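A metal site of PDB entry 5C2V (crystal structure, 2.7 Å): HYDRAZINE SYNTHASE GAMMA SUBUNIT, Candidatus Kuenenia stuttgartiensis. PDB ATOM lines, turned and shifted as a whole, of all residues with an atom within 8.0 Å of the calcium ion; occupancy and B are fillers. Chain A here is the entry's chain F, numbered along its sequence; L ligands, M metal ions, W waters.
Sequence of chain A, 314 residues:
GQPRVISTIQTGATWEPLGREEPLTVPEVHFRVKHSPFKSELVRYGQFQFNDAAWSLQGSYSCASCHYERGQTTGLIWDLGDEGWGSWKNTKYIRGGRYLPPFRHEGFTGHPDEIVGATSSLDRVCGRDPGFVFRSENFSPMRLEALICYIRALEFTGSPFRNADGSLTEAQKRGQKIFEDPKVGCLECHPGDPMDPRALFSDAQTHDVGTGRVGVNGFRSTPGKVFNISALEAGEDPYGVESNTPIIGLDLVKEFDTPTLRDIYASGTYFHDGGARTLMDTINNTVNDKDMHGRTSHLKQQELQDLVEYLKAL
The backbone NH (N) of Arg 104 sits at hydrogen-bond distance from an oxygen (O1) of the ligand (2.6 Å). NE of Arg 104 lies within salt-bridge range of O4 of the ligand (2.7 Å). An oxygen (O3) of the ligand lies close to the backbone NH of His 105. A ring nitrogen (ND1) of His 105 is in hydrogen-bond range of an oxygen (O3) of the ligand, 2.7 Å away.
OD2 of Asp 257 is bound to the calcium ion (2.4 Å). The calcium ion is bound by water W3 (2.4 Å). The calcium ion is bound by the backbone carbonyl oxygen (O) of Pro 102. The calcium ion is bound by water W1, at 2.4 Å. The backbone carbonyl oxygen (O) of Leu 100 binds the calcium ion (2.9 Å). Slightly farther from the calcium ion lies water W2 (3.0 Å).
Three residues have an atom within 4 Å of the calcium ion: Leu 100, Pro 102 and Asp 257. The nearest printed residue that does not touch the calcium ion is Phe 103 (4.3 Å).
Water W2 lies within hydrogen-bond range of the backbone NH of Arg 104, the side-chain amino group of Lys 92 and an oxygen (O2) of the ligand.
N of Asp 257 lies within hydrogen-bond range of O of His 105, 2.7 Å away.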
ATOM      1  N   LYS A  92      24.853   3.219 -20.225  1.00  0.00           N
ATOM      2  CA  LYS A  92      25.501   4.523 -20.118  1.00  0.00           C
ATOM      3  C   LYS A  92      25.875   4.900 -18.695  1.00  0.00           C
ATOM      4  O   LYS A  92      25.221   4.496 -17.731  1.00  0.00           O
ATOM      5  CB  LYS A  92      24.607   5.609 -20.718  1.00  0.00           C
ATOM      6  CG  LYS A  92      24.924   5.962 -22.159  1.00  0.00           C
ATOM      7  CD  LYS A  92      26.240   6.714 -22.260  1.00  0.00           C
ATOM      8  CE  LYS A  92      26.480   7.228 -23.676  1.00  0.00           C
ATOM      9  NZ  LYS A  92      27.791   7.913 -23.798  1.00  0.00           N
ATOM     10  N   GLY A  96      27.225  13.141 -14.305  1.00  0.00           N
ATOM     11  CA  GLY A  96      27.625  14.285 -15.109  1.00  0.00           C
ATOM     12  C   GLY A  96      27.139  14.200 -16.539  1.00  0.00           C
ATOM     13  O   GLY A  96      27.932  14.300 -17.484  1.00  0.00           O
ATOM     14  N   GLY A  97      25.835  14.022 -16.710  1.00  0.00           N
ATOM     15  CA  GLY A  97      25.240  13.940 -18.033  1.00  0.00           C
ATOM     16  C   GLY A  97      24.745  15.276 -18.546  1.00  0.00           C
ATOM     17  O   GLY A  97      24.574  15.455 -19.749  1.00  0.00           O
ATOM     18  N   TYR A  99      26.251  17.997 -18.697  1.00  0.00           N
ATOM     19  CA  TYR A  99      27.315  18.821 -19.261  1.00  0.00           C
ATOM     20  C   TYR A  99      27.590  18.548 -20.729  1.00  0.00           C
ATOM     21  O   TYR A  99      28.304  19.318 -21.378  1.00  0.00           O
ATOM     22  CB  TYR A  99      28.600  18.639 -18.453  1.00  0.00           C
ATOM     23  CG  TYR A  99      28.450  18.931 -16.975  1.00  0.00           C
ATOM     24  CD1 TYR A  99      28.358  20.233 -16.513  1.00  0.00           C
ATOM     25  CD2 TYR A  99      28.418  17.893 -16.043  1.00  0.00           C
ATOM     26  CE1 TYR A  99      28.225  20.498 -15.168  1.00  0.00           C
ATOM     27  CE2 TYR A  99      28.286  18.157 -14.697  1.00  0.00           C
ATOM     28  CZ  TYR A  99      28.190  19.460 -14.260  1.00  0.00           C
ATOM     29  OH  TYR A  99      28.060  19.734 -12.918  1.00  0.00           O
ATOM     30  N   LEU A 100      27.055  17.458 -21.261  1.00  0.00           N
ATOM     31  CA  LEU A 100      27.400  17.058 -22.624  1.00  0.00           C
ATOM     32  C   LEU A 100      26.234  16.540 -23.473  1.00  0.00           C
ATOM     33  O   LEU A 100      26.049  15.341 -23.632  1.00  0.00           O
ATOM     34  CB  LEU A 100      28.481  15.970 -22.582  1.00  0.00           C
ATOM     35  CG  LEU A 100      29.883  16.444 -22.213  1.00  0.00           C
ATOM     36  CD1 LEU A 100      30.764  15.276 -21.823  1.00  0.00           C
ATOM     37  CD2 LEU A 100      30.502  17.222 -23.367  1.00  0.00           C
ATOM     38  N   PRO A 101      25.428  17.470 -24.018  1.00  0.00           N
ATOM     39  CA  PRO A 101      24.455  17.116 -25.055  1.00  0.00           C
ATOM     40  C   PRO A 101      25.166  16.907 -26.395  1.00  0.00           C
ATOM     41  O   PRO A 101      26.222  17.492 -26.596  1.00  0.00           O
ATOM     42  CB  PRO A 101      23.520  18.332 -25.110  1.00  0.00           C
ATOM     43  CG  PRO A 101      23.821  19.120 -23.870  1.00  0.00           C
ATOM     44  CD  PRO A 101      25.260  18.864 -23.574  1.00  0.00           C
ATOM     45  N   PRO A 102      24.593  16.085 -27.302  1.00  0.00           N
ATOM     46  CA  PRO A 102      23.360  15.299 -27.180  1.00  0.00           C
ATOM     47  C   PRO A 102      23.562  14.022 -26.366  1.00  0.00           C
ATOM     48  O   PRO A 102      24.597  13.861 -25.715  1.00  0.00           O
ATOM     49  CB  PRO A 102      23.032  14.960 -28.640  1.00  0.00           C
ATOM     50  CG  PRO A 102      24.353  14.882 -29.296  1.00  0.00           C
ATOM     51  CD  PRO A 102      25.203  15.936 -28.624  1.00  0.00           C
ATOM     52  N   PHE A 103      22.579  13.126 -26.396  1.00  0.00           N
ATOM     53  CA  PHE A 103      22.559  12.014 -25.467  1.00  0.00           C
ATOM     54  C   PHE A 103      22.535  10.618 -26.103  1.00  0.00           C
ATOM     55  O   PHE A 103      22.316  10.460 -27.311  1.00  0.00           O
ATOM     56  CB  PHE A 103      21.369  12.157 -24.503  1.00  0.00           C
ATOM     57  CG  PHE A 103      21.401  13.436 -23.707  1.00  0.00           C
ATOM     58  CD1 PHE A 103      22.334  13.614 -22.695  1.00  0.00           C
ATOM     59  CD2 PHE A 103      20.495  14.451 -23.958  1.00  0.00           C
ATOM     60  CE1 PHE A 103      22.376  14.792 -21.957  1.00  0.00           C
ATOM     61  CE2 PHE A 103      20.527  15.629 -23.222  1.00  0.00           C
ATOM     62  CZ  PHE A 103      21.461  15.789 -22.223  1.00  0.00           C
ATOM     63  N   ARG A 104      22.780   9.638 -25.251  1.00  0.00           N
ATOM     64  CA  ARG A 104      23.153   8.252 -25.551  1.00  0.00           C
ATOM     65  C   ARG A 104      24.412   8.122 -26.407  1.00  0.00           C
ATOM     66  O   ARG A 104      25.273   9.009 -26.392  1.00  0.00           O
ATOM     67  CB  ARG A 104      21.982   7.542 -26.236  1.00  0.00           C
ATOM     68  CG  ARG A 104      20.731   7.440 -25.377  1.00  0.00           C
ATOM     69  CD  ARG A 104      19.456   7.232 -26.197  1.00  0.00           C
ATOM     70  NE  ARG A 104      19.480   6.004 -26.977  1.00  0.00           N
ATOM     71  CZ  ARG A 104      18.453   5.150 -27.060  1.00  0.00           C
ATOM     72  NH1 ARG A 104      17.339   5.401 -26.387  1.00  0.00           N
ATOM     73  NH2 ARG A 104      18.560   4.059 -27.799  1.00  0.00           N
ATOM     74  N   HIS A 105      24.520   7.027 -27.155  1.00  0.00           N
ATOM     75  CA  HIS A 105      25.748   6.736 -27.892  1.00  0.00           C
ATOM     76  C   HIS A 105      25.806   7.254 -29.327  1.00  0.00           C
ATOM     77  O   HIS A 105      26.819   7.802 -29.757  1.00  0.00           O
ATOM     78  CB  HIS A 105      26.015   5.233 -27.866  1.00  0.00           C
ATOM     79  CG  HIS A 105      26.542   4.751 -26.552  1.00  0.00           C
ATOM     80  ND1 HIS A 105      25.739   4.210 -25.571  1.00  0.00           N
ATOM     81  CD2 HIS A 105      27.800   4.759 -26.039  1.00  0.00           C
ATOM     82  CE1 HIS A 105      26.478   3.892 -24.522  1.00  0.00           C
ATOM     83  NE2 HIS A 105      27.728   4.214 -24.776  1.00  0.00           N
ATOM     84  N   GLU A 106      24.711   7.079 -30.056  1.00  0.00           N
ATOM     85  CA  GLU A 106      24.706   7.371 -31.492  1.00  0.00           C
ATOM     86  C   GLU A 106      24.604   8.870 -31.731  1.00  0.00           C
ATOM     87  O   GLU A 106      23.999   9.595 -30.950  1.00  0.00           O
ATOM     88  CB  GLU A 106      23.563   6.626 -32.187  1.00  0.00           C
ATOM     89  CG  GLU A 106      23.555   5.134 -31.877  1.00  0.00           C
ATOM     90  CD  GLU A 106      22.879   4.308 -32.960  1.00  0.00           C
ATOM     91  OE1 GLU A 106      22.967   3.066 -32.901  1.00  0.00           O
ATOM     92  OE2 GLU A 106      22.249   4.914 -33.863  1.00  0.00           O
ATOM     93  N   ALA A 118      21.701  10.896 -31.077  1.00  0.00           N
ATOM     94  CA  ALA A 118      21.788  12.353 -30.962  1.00  0.00           C
ATOM     95  C   ALA A 118      20.581  12.926 -30.229  1.00  0.00           C
ATOM     96  O   ALA A 118      19.995  13.915 -30.656  1.00  0.00           O
ATOM     97  CB  ALA A 118      21.912  12.984 -32.346  1.00  0.00           C
ATOM     98  N   THR A 119      20.223  12.281 -29.130  1.00  0.00           N
ATOM     99  CA  THR A 119      19.023  12.654 -28.376  1.00  0.00           C
ATOM    100  C   THR A 119      19.127  14.086 -27.874  1.00  0.00           C
ATOM    101  O   THR A 119      20.081  14.438 -27.187  1.00  0.00           O
ATOM    102  CB  THR A 119      18.790  11.702 -27.201  1.00  0.00           C
ATOM    103  OG1 THR A 119      19.068  10.360 -27.599  1.00  0.00           O
ATOM    104  CG2 THR A 119      17.348  11.786 -26.731  1.00  0.00           C
ATOM    105  N   SER A 202      35.605  15.970 -23.644  1.00  0.00           N
ATOM    106  CA  SER A 202      34.768  15.474 -24.729  1.00  0.00           C
ATOM    107  C   SER A 202      34.502  16.522 -25.796  1.00  0.00           C
ATOM    108  O   SER A 202      34.328  17.703 -25.500  1.00  0.00           O
ATOM    109  CB  SER A 202      33.436  14.951 -24.168  1.00  0.00           C
ATOM    110  OG  SER A 202      32.573  14.536 -25.222  1.00  0.00           O
ATOM    111  N   ALA A 204      31.901  16.404 -27.737  1.00  0.00           N
ATOM    112  CA  ALA A 204      30.443  16.516 -27.829  1.00  0.00           C
ATOM    113  C   ALA A 204      29.979  16.553 -29.278  1.00  0.00           C
ATOM    114  O   ALA A 204      28.975  17.184 -29.608  1.00  0.00           O
ATOM    115  CB  ALA A 204      29.946  17.745 -27.068  1.00  0.00           C
ATOM    116  N   GLN A 205      30.723  15.866 -30.139  1.00  0.00           N
ATOM    117  CA  GLN A 205      30.404  15.797 -31.563  1.00  0.00           C
ATOM    118  C   GLN A 205      30.383  14.349 -32.031  1.00  0.00           C
ATOM    119  O   GLN A 205      30.503  13.423 -31.229  1.00  0.00           O
ATOM    120  CB  GLN A 205      31.414  16.608 -32.383  1.00  0.00           C
ATOM    121  CG  GLN A 205      31.441  18.090 -32.048  1.00  0.00           C
ATOM    122  CD  GLN A 205      32.489  18.846 -32.843  1.00  0.00           C
ATOM    123  OE1 GLN A 205      32.988  18.364 -33.858  1.00  0.00           O
ATOM    124  NE2 GLN A 205      32.844  20.038 -32.363  1.00  0.00           N
ATOM    125  N   ASP A 257      28.506   9.555 -30.842  1.00  0.00           N
ATOM    126  CA  ASP A 257      28.761  10.747 -30.032  1.00  0.00           C
ATOM    127  C   ASP A 257      29.929  10.511 -29.074  1.00  0.00           C
ATOM    128  O   ASP A 257      30.034   9.445 -28.463  1.00  0.00           O
ATOM    129  CB  ASP A 257      27.510  11.155 -29.260  1.00  0.00           C
ATOM    130  CG  ASP A 257      27.685  12.471 -28.520  1.00  0.00           C
ATOM    131  OD1 ASP A 257      28.274  13.409 -29.109  1.00  0.00           O
ATOM    132  OD2 ASP A 257      27.226  12.583 -27.373  1.00  0.00           O
ATOM    133  N   THR A 258      30.788  11.518 -28.941  1.00  0.00           N
ATOM    134  CA  THR A 258      31.967  11.396 -28.091  1.00  0.00           C
ATOM    135  C   THR A 258      31.611  11.492 -26.607  1.00  0.00           C
ATOM    136  O   THR A 258      31.125  12.522 -26.138  1.00  0.00           O
ATOM    137  CB  THR A 258      33.002  12.489 -28.417  1.00  0.00           C
ATOM    138  OG1 THR A 258      33.410  12.369 -29.787  1.00  0.00           O
ATOM    139  CG2 THR A 258      34.221  12.358 -27.521  1.00  0.00           C
ATOM    140  N   PRO A 259      31.855  10.403 -25.856  1.00  0.00           N
ATOM    141  CA  PRO A 259      31.597  10.312 -24.413  1.00  0.00           C
ATOM    142  C   PRO A 259      32.680  11.000 -23.591  1.00  0.00           C
ATOM    143  O   PRO A 259      33.791  11.194 -24.074  1.00  0.00           O
ATOM    144  CB  PRO A 259      31.577   8.799 -24.151  1.00  0.00           C
ATOM    145  CG  PRO A 259      31.894   8.128 -25.471  1.00  0.00           C
ATOM    146  CD  PRO A 259      32.477   9.168 -26.361  1.00  0.00           C
ATOM    147  N   THR A 260      32.350  11.365 -22.357  1.00  0.00           N
ATOM    148  CA  THR A 260      33.310  11.976 -21.455  1.00  0.00           C
ATOM    149  C   THR A 260      34.348  10.976 -20.971  1.00  0.00           C
ATOM    150  O   THR A 260      34.068   9.775 -20.867  1.00  0.00           O
ATOM    151  CB  THR A 260      32.612  12.598 -20.226  1.00  0.00           C
ATOM    152  OG1 THR A 260      33.598  13.183 -19.363  1.00  0.00           O
ATOM    153  CG2 THR A 260      31.831  11.545 -19.465  1.00  0.00           C
HETATM  154 FE1  LIG L   1      19.173   3.973 -19.533  1.00  0.00          FE
HETATM  155  C1  LIG L   1      21.242   5.376 -21.887  1.00  0.00           C
HETATM  156  C2  LIG L   1      18.605   7.067 -18.194  1.00  0.00           C
HETATM  157  C3  LIG L   1      16.820   2.631 -17.387  1.00  0.00           C
HETATM  158  C4  LIG L   1      20.184   0.833 -20.370  1.00  0.00           C
HETATM  159  N1  LIG L   1      19.776   5.886 -19.993  1.00  0.00           N
HETATM  160  C5  LIG L   1      20.710   6.237 -20.939  1.00  0.00           C
HETATM  161  C6  LIG L   1      21.033   7.643 -20.757  1.00  0.00           C
HETATM  162  C7  LIG L   1      20.300   8.095 -19.740  1.00  0.00           C
HETATM  163  C8  LIG L   1      19.494   7.007 -19.242  1.00  0.00           C
HETATM  164  C9  LIG L   1      20.272   9.534 -19.160  1.00  0.00           C
HETATM  165  C10 LIG L   1      22.034   8.454 -21.625  1.00  0.00           C
HETATM  166  C11 LIG L   1      23.248   8.902 -20.798  1.00  0.00           C
HETATM  167  C12 LIG L   1      24.183   9.719 -21.645  1.00  0.00           C
HETATM  168  O1  LIG L   1      23.937   9.831 -22.881  1.00  0.00           O
HETATM  169  O2  LIG L   1      25.176  10.254 -21.099  1.00  0.00           O
HETATM  170  N2  LIG L   1      18.005   4.694 -17.974  1.00  0.00           N
HETATM  171  C13 LIG L   1      17.793   6.037 -17.763  1.00  0.00           C
HETATM  172  C14 LIG L   1      16.561   6.189 -17.007  1.00  0.00           C
HETATM  173  C15 LIG L   1      16.070   4.962 -16.773  1.00  0.00           C
HETATM  174  C16 LIG L   1      16.964   4.002 -17.388  1.00  0.00           C
HETATM  175  C17 LIG L   1      15.957   7.534 -16.549  1.00  0.00           C
HETATM  176  C18 LIG L   1      14.775   4.598 -16.018  1.00  0.00           C
HETATM  177  C19 LIG L   1      13.524   5.015 -16.824  1.00  0.00           C
HETATM  178  N3  LIG L   1      18.619   2.080 -18.961  1.00  0.00           N
HETATM  179  C20 LIG L   1      17.601   1.737 -18.091  1.00  0.00           C
HETATM  180  C21 LIG L   1      17.397   0.314 -18.175  1.00  0.00           C
HETATM  181  C22 LIG L   1      18.420  -0.195 -18.881  1.00  0.00           C
HETATM  182  C23 LIG L   1      19.147   0.913 -19.473  1.00  0.00           C
HETATM  183  C24 LIG L   1      16.488  -0.482 -17.208  1.00  0.00           C
HETATM  184  C25 LIG L   1      18.679  -1.691 -19.161  1.00  0.00           C
HETATM  185  C26 LIG L   1      17.581  -2.251 -20.103  1.00  0.00           C
HETATM  186  N4  LIG L   1      20.577   3.229 -20.879  1.00  0.00           N
HETATM  187  C27 LIG L   1      20.658   1.858 -21.165  1.00  0.00           C
HETATM  188  C28 LIG L   1      21.327   1.696 -22.435  1.00  0.00           C
HETATM  189  C29 LIG L   1      21.656   3.121 -22.910  1.00  0.00           C
HETATM  190  C30 LIG L   1      21.158   4.005 -21.877  1.00  0.00           C
HETATM  191  C31 LIG L   1      21.636   0.373 -23.162  1.00  0.00           C
HETATM  192  C32 LIG L   1      22.375   3.526 -24.222  1.00  0.00           C
HETATM  193  C33 LIG L   1      21.332   3.751 -25.315  1.00  0.00           C
HETATM  194  C34 LIG L   1      22.033   3.964 -26.627  1.00  0.00           C
HETATM  195  O3  LIG L   1      23.287   3.890 -26.659  1.00  0.00           O
HETATM  196  O4  LIG L   1      21.340   4.212 -27.652  1.00  0.00           O
HETATM  197 CA    CA M   1      26.720  12.976 -25.096  1.00  0.00          CA
HETATM  198  O   HOH W   1      26.163  13.282 -22.789  1.00  0.00           O
HETATM  199  O   HOH W   2      25.606  10.266 -24.494  1.00  0.00           O
HETATM  200  O   HOH W   3      28.877  12.203 -24.464  1.00  0.00           O
